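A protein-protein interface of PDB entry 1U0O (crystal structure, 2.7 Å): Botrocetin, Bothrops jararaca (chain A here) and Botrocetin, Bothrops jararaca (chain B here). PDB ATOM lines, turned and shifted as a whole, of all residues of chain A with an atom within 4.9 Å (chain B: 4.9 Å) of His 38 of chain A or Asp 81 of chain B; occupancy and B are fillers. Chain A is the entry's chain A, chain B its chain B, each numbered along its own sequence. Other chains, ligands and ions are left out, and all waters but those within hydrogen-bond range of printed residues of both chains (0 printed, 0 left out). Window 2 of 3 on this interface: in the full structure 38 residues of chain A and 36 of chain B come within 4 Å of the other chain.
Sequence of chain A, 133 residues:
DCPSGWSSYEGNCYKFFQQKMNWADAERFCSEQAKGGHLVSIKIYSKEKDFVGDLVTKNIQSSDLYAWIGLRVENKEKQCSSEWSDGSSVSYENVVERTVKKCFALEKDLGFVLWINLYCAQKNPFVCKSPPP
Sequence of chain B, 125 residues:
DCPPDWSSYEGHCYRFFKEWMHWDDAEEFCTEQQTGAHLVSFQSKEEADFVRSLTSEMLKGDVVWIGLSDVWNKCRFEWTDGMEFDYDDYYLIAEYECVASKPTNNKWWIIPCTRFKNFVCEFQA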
ATOM      1  N   GLU A  27     -10.079  -2.921  -8.541  1.00  0.00           N
ATOM      2  CA  GLU A  27     -10.875  -1.915  -9.224  1.00  0.00           C
ATOM      3  C   GLU A  27      -9.965  -0.848  -9.813  1.00  0.00           C
ATOM      4  O   GLU A  27     -10.128  -0.460 -10.967  1.00  0.00           O
ATOM      5  CB  GLU A  27     -11.876  -1.292  -8.248  1.00  0.00           C
ATOM      6  CG  GLU A  27     -12.374   0.093  -8.639  1.00  0.00           C
ATOM      7  CD  GLU A  27     -13.236   0.108  -9.883  1.00  0.00           C
ATOM      8  OE1 GLU A  27     -13.331  -0.931 -10.574  1.00  0.00           O
ATOM      9  OE2 GLU A  27     -13.814   1.177 -10.172  1.00  0.00           O
ATOM     10  N   CYS A  30      -8.258  -1.928 -12.847  1.00  0.00           N
ATOM     11  CA  CYS A  30      -9.084  -1.981 -14.046  1.00  0.00           C
ATOM     12  C   CYS A  30      -9.226  -0.583 -14.649  1.00  0.00           C
ATOM     13  O   CYS A  30      -9.293  -0.427 -15.867  1.00  0.00           O
ATOM     14  CB  CYS A  30     -10.477  -2.510 -13.736  1.00  0.00           C
ATOM     15  SG  CYS A  30     -10.624  -4.238 -13.213  1.00  0.00           S
ATOM     16  N   SER A  31      -9.298   0.434 -13.797  1.00  0.00           N
ATOM     17  CA  SER A  31      -9.427   1.796 -14.292  1.00  0.00           C
ATOM     18  C   SER A  31      -8.031   2.343 -14.541  1.00  0.00           C
ATOM     19  O   SER A  31      -7.737   3.507 -14.270  1.00  0.00           O
ATOM     20  CB  SER A  31     -10.179   2.675 -13.286  1.00  0.00           C
ATOM     21  OG  SER A  31      -9.440   2.839 -12.091  1.00  0.00           O
ATOM     22  N   GLY A  36     -12.071   3.925 -19.139  1.00  0.00           N
ATOM     23  CA  GLY A  36     -13.418   3.581 -18.726  1.00  0.00           C
ATOM     24  C   GLY A  36     -13.565   2.115 -18.392  1.00  0.00           C
ATOM     25  O   GLY A  36     -14.456   1.440 -18.899  1.00  0.00           O
ATOM     26  N   GLY A  37     -12.683   1.614 -17.539  1.00  0.00           N
ATOM     27  CA  GLY A  37     -12.746   0.216 -17.163  1.00  0.00           C
ATOM     28  C   GLY A  37     -12.752   0.046 -15.659  1.00  0.00           C
ATOM     29  O   GLY A  37     -12.155   0.843 -14.937  1.00  0.00           O
ATOM     30  N   HIS A  38     -13.456  -0.979 -15.186  1.00  0.00           N
ATOM     31  CA  HIS A  38     -13.541  -1.284 -13.754  1.00  0.00           C
ATOM     32  C   HIS A  38     -13.745  -2.782 -13.625  1.00  0.00           C
ATOM     33  O   HIS A  38     -13.571  -3.525 -14.589  1.00  0.00           O
ATOM     34  CB  HIS A  38     -14.736  -0.587 -13.100  1.00  0.00           C
ATOM     35  CG  HIS A  38     -15.074   0.732 -13.710  1.00  0.00           C
ATOM     36  ND1 HIS A  38     -14.944   1.921 -13.027  1.00  0.00           N
ATOM     37  CD2 HIS A  38     -15.534   1.050 -14.943  1.00  0.00           C
ATOM     38  CE1 HIS A  38     -15.309   2.916 -13.815  1.00  0.00           C
ATOM     39  NE2 HIS A  38     -15.670   2.414 -14.982  1.00  0.00           N
ATOM     40  N   LEU A  39     -14.106  -3.220 -12.424  1.00  0.00           N
ATOM     41  CA  LEU A  39     -14.371  -4.634 -12.199  1.00  0.00           C
ATOM     42  C   LEU A  39     -15.635  -4.934 -13.006  1.00  0.00           C
ATOM     43  O   LEU A  39     -16.596  -4.164 -12.973  1.00  0.00           O
ATOM     44  CB  LEU A  39     -14.626  -4.889 -10.720  1.00  0.00           C
ATOM     45  CG  LEU A  39     -13.472  -4.599  -9.767  1.00  0.00           C
ATOM     46  CD1 LEU A  39     -14.034  -4.260  -8.407  1.00  0.00           C
ATOM     47  CD2 LEU A  39     -12.549  -5.784  -9.690  1.00  0.00           C
ATOM     48  N   VAL A  40     -15.623  -6.032 -13.746  1.00  0.00           N
ATOM     49  CA  VAL A  40     -16.768  -6.413 -14.559  1.00  0.00           C
ATOM     50  C   VAL A  40     -18.098  -6.123 -13.850  1.00  0.00           C
ATOM     51  O   VAL A  40     -18.173  -6.094 -12.626  1.00  0.00           O
ATOM     52  CB  VAL A  40     -16.688  -7.923 -14.924  1.00  0.00           C
ATOM     53  CG1 VAL A  40     -16.924  -8.793 -13.682  1.00  0.00           C
ATOM     54  CG2 VAL A  40     -17.688  -8.248 -16.010  1.00  0.00           C
ATOM     55  N   SER A  41     -19.143  -5.891 -14.633  1.00  0.00           N
ATOM     56  CA  SER A  41     -20.470  -5.627 -14.084  1.00  0.00           C
ATOM     57  C   SER A  41     -21.395  -6.623 -14.769  1.00  0.00           C
ATOM     58  O   SER A  41     -21.373  -6.746 -15.996  1.00  0.00           O
ATOM     59  CB  SER A  41     -20.904  -4.201 -14.399  1.00  0.00           C
ATOM     60  OG  SER A  41     -21.064  -4.008 -15.795  1.00  0.00           O
ATOM     61  N   VAL A 127     -11.957 -10.023 -12.811  1.00  0.00           N
ATOM     62  CA  VAL A 127     -12.301  -9.754 -14.198  1.00  0.00           C
ATOM     63  C   VAL A 127     -12.531  -8.241 -14.338  1.00  0.00           C
ATOM     64  O   VAL A 127     -13.224  -7.626 -13.518  1.00  0.00           O
ATOM     65  CB  VAL A 127     -13.580 -10.524 -14.628  1.00  0.00           C
ATOM     66  CG1 VAL A 127     -13.968 -10.151 -16.056  1.00  0.00           C
ATOM     67  CG2 VAL A 127     -13.337 -12.017 -14.534  1.00  0.00           C
ATOM     68  N   CYS A 128     -11.909  -7.649 -15.361  1.00  0.00           N
ATOM     69  CA  CYS A 128     -12.034  -6.218 -15.643  1.00  0.00           C
ATOM     70  C   CYS A 128     -12.961  -6.032 -16.840  1.00  0.00           C
ATOM     71  O   CYS A 128     -13.094  -6.923 -17.679  1.00  0.00           O
ATOM     72  CB  CYS A 128     -10.666  -5.595 -15.958  1.00  0.00           C
ATOM     73  SG  CYS A 128      -9.527  -5.303 -14.551  1.00  0.00           S
ATOM     74  N   LYS A 129     -13.601  -4.872 -16.919  1.00  0.00           N
ATOM     75  CA  LYS A 129     -14.519  -4.588 -18.016  1.00  0.00           C
ATOM     76  C   LYS A 129     -14.342  -3.152 -18.503  1.00  0.00           C
ATOM     77  O   LYS A 129     -13.998  -2.257 -17.728  1.00  0.00           O
ATOM     78  CB  LYS A 129     -15.968  -4.815 -17.565  1.00  0.00           C
ATOM     79  CG  LYS A 129     -17.008  -4.669 -18.664  1.00  0.00           C
ATOM     80  CD  LYS A 129     -18.411  -4.788 -18.102  1.00  0.00           C
ATOM     81  CE  LYS A 129     -19.467  -4.598 -19.177  1.00  0.00           C
ATOM     82  NZ  LYS A 129     -20.860  -4.640 -18.623  1.00  0.00           N
ATOM     83  N   TRP B  79     -22.623  -0.524  -8.690  1.00  0.00           N
ATOM     84  CA  TRP B  79     -21.460  -1.025  -9.385  1.00  0.00           C
ATOM     85  C   TRP B  79     -20.484   0.097  -9.636  1.00  0.00           C
ATOM     86  O   TRP B  79     -20.858   1.275  -9.631  1.00  0.00           O
ATOM     87  CB  TRP B  79     -21.854  -1.639 -10.723  1.00  0.00           C
ATOM     88  CG  TRP B  79     -22.807  -2.765 -10.623  1.00  0.00           C
ATOM     89  CD1 TRP B  79     -24.164  -2.688 -10.520  1.00  0.00           C
ATOM     90  CD2 TRP B  79     -22.481  -4.155 -10.673  1.00  0.00           C
ATOM     91  NE1 TRP B  79     -24.708  -3.950 -10.516  1.00  0.00           N
ATOM     92  CE2 TRP B  79     -23.696  -4.869 -10.607  1.00  0.00           C
ATOM     93  CE3 TRP B  79     -21.277  -4.866 -10.767  1.00  0.00           C
ATOM     94  CZ2 TRP B  79     -23.744  -6.263 -10.634  1.00  0.00           C
ATOM     95  CZ3 TRP B  79     -21.323  -6.244 -10.792  1.00  0.00           C
ATOM     96  CH2 TRP B  79     -22.553  -6.932 -10.725  1.00  0.00           C
ATOM     97  N   THR B  80     -19.227  -0.273  -9.846  1.00  0.00           N
ATOM     98  CA  THR B  80     -18.200   0.711 -10.135  1.00  0.00           C
ATOM     99  C   THR B  80     -18.496   1.381 -11.487  1.00  0.00           C
ATOM    100  O   THR B  80     -18.319   2.587 -11.645  1.00  0.00           O
ATOM    101  CB  THR B  80     -16.823   0.050 -10.180  1.00  0.00           C
ATOM    102  OG1 THR B  80     -16.900  -1.141 -10.968  1.00  0.00           O
ATOM    103  CG2 THR B  80     -16.359  -0.305  -8.783  1.00  0.00           C
ATOM    104  N   ASP B  81     -18.963   0.608 -12.460  1.00  0.00           N
ATOM    105  CA  ASP B  81     -19.260   1.181 -13.771  1.00  0.00           C
ATOM    106  C   ASP B  81     -20.593   1.936 -13.747  1.00  0.00           C
ATOM    107  O   ASP B  81     -21.074   2.406 -14.782  1.00  0.00           O
ATOM    108  CB  ASP B  81     -19.290   0.078 -14.840  1.00  0.00           C
ATOM    109  CG  ASP B  81     -20.586  -0.709 -14.840  1.00  0.00           C
ATOM    110  OD1 ASP B  81     -21.174  -0.915 -13.755  1.00  0.00           O
ATOM    111  OD2 ASP B  81     -21.013  -1.139 -15.932  1.00  0.00           O
ATOM    112  N   GLY B  82     -21.181   2.048 -12.555  1.00  0.00           N
ATOM    113  CA  GLY B  82     -22.442   2.753 -12.398  1.00  0.00           C
ATOM    114  C   GLY B  82     -23.623   2.157 -13.144  1.00  0.00           C
ATOM    115  O   GLY B  82     -24.590   2.849 -13.451  1.00  0.00           O
ATOM    116  N   MET B  83     -23.560   0.867 -13.431  1.00  0.00           N
ATOM    117  CA  MET B  83     -24.635   0.199 -14.141  1.00  0.00           C
ATOM    118  C   MET B  83     -25.974   0.306 -13.393  1.00  0.00           C
ATOM    119  O   MET B  83     -26.020   0.293 -12.159  1.00  0.00           O
ATOM    120  CB  MET B  83     -24.264  -1.265 -14.353  1.00  0.00           C
ATOM    121  CG  MET B  83     -25.237  -2.014 -15.194  1.00  0.00           C
ATOM    122  SD  MET B  83     -24.890  -3.773 -15.167  1.00  0.00           S
ATOM    123  CE  MET B  83     -25.959  -4.285 -13.769  1.00  0.00           C
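OG of Ser 41 of chain A is in hydrogen-bond range of OD2 of Asp 81 of chain B, 2.9 Å away.
A ring nitrogen (ND1) of His 38 of chain A lies within hydrogen-bond range of the side-chain carboxylate (OE2) of Glu 27 of chain A (3.2 Å).
The backbone NH (N) of Leu 39 of chain A sits at hydrogen-bond distance from the side-chain sulfur (SG) of Cys 30 of chain A.
The backbone carbonyl oxygen (O) of His 38 of chain A is in hydrogen-bond range of the backbone NH (N) of Lys 129 of chain A, at 2.7 Å.
The backbone carbonyl oxygen (O) of Val 127 of chain A is in hydrogen-bond range of the backbone NH (N) of Val 40 of chain A.
The side-chain hydroxyl (OG) of Ser 41 of chain A sits at hydrogen-bond distance from the side-chain amino group (NZ) of Lys 129 of chain A, 2.9 Å away.
The backbone NH (N) of Met 83 of chain B sits at hydrogen-bond distance from the side-chain carboxylate (OD1) of Asp 81 of chain B (3.0 Å).
Glu 27 of chain A touches Thr 80 of chain B.
Thr 80 of chain B touches His 38 of chain A.
His 38 of chain A touches Asp 81 of chain B.
O of Leu 39 of chain A touches OG1 of Thr 80 of chain B, 3.6 Å away.
O of Val 40 of chain A touches CZ3 of Trp 79 of chain B, at 3.6 Å.
Trp 79 of chain B touches Ser 41 of chain A.
Met 83 of chain B touches Ser 41 of chain A.
Of chain B, only Thr 80 (3.1 Å) and Asp 81 (3.9 Å) come within 4 Å of His 38 of chain A.
Printed residues of chain A within 4 Å of Asp 81 of chain B: His 38 (3.9 Å) and Ser 41 (2.9 Å).
Printed residues of chain A within 4 Å of Thr 80 of chain B: Glu 27, His 38 and Leu 39.
Printed residues of chain A within 4 Å of Trp 79 of chain B: Val 40 (3.6 Å) and Ser 41 (3.5 Å).
Of the printed residues of chain B, Glu 27 of chain A touches Thr 80.
Of the 5 printed residues of chain B, 4 touch a printed residue of chain A.
Printed residues of chain B that touch a printed residue of chain A: Trp 79, Thr 80, Asp 81 and Met 83.
Hydrophobic or aromatic side chains of chain B that line the printed part of chain A: Trp 79 and Met 83.
Among the printed residues, 8 pairs touch across the chains.
Among the printed residues, no Asp or Glu carboxylate lies within 4 Å of a Lys or Arg side-chain nitrogen of the other chain.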
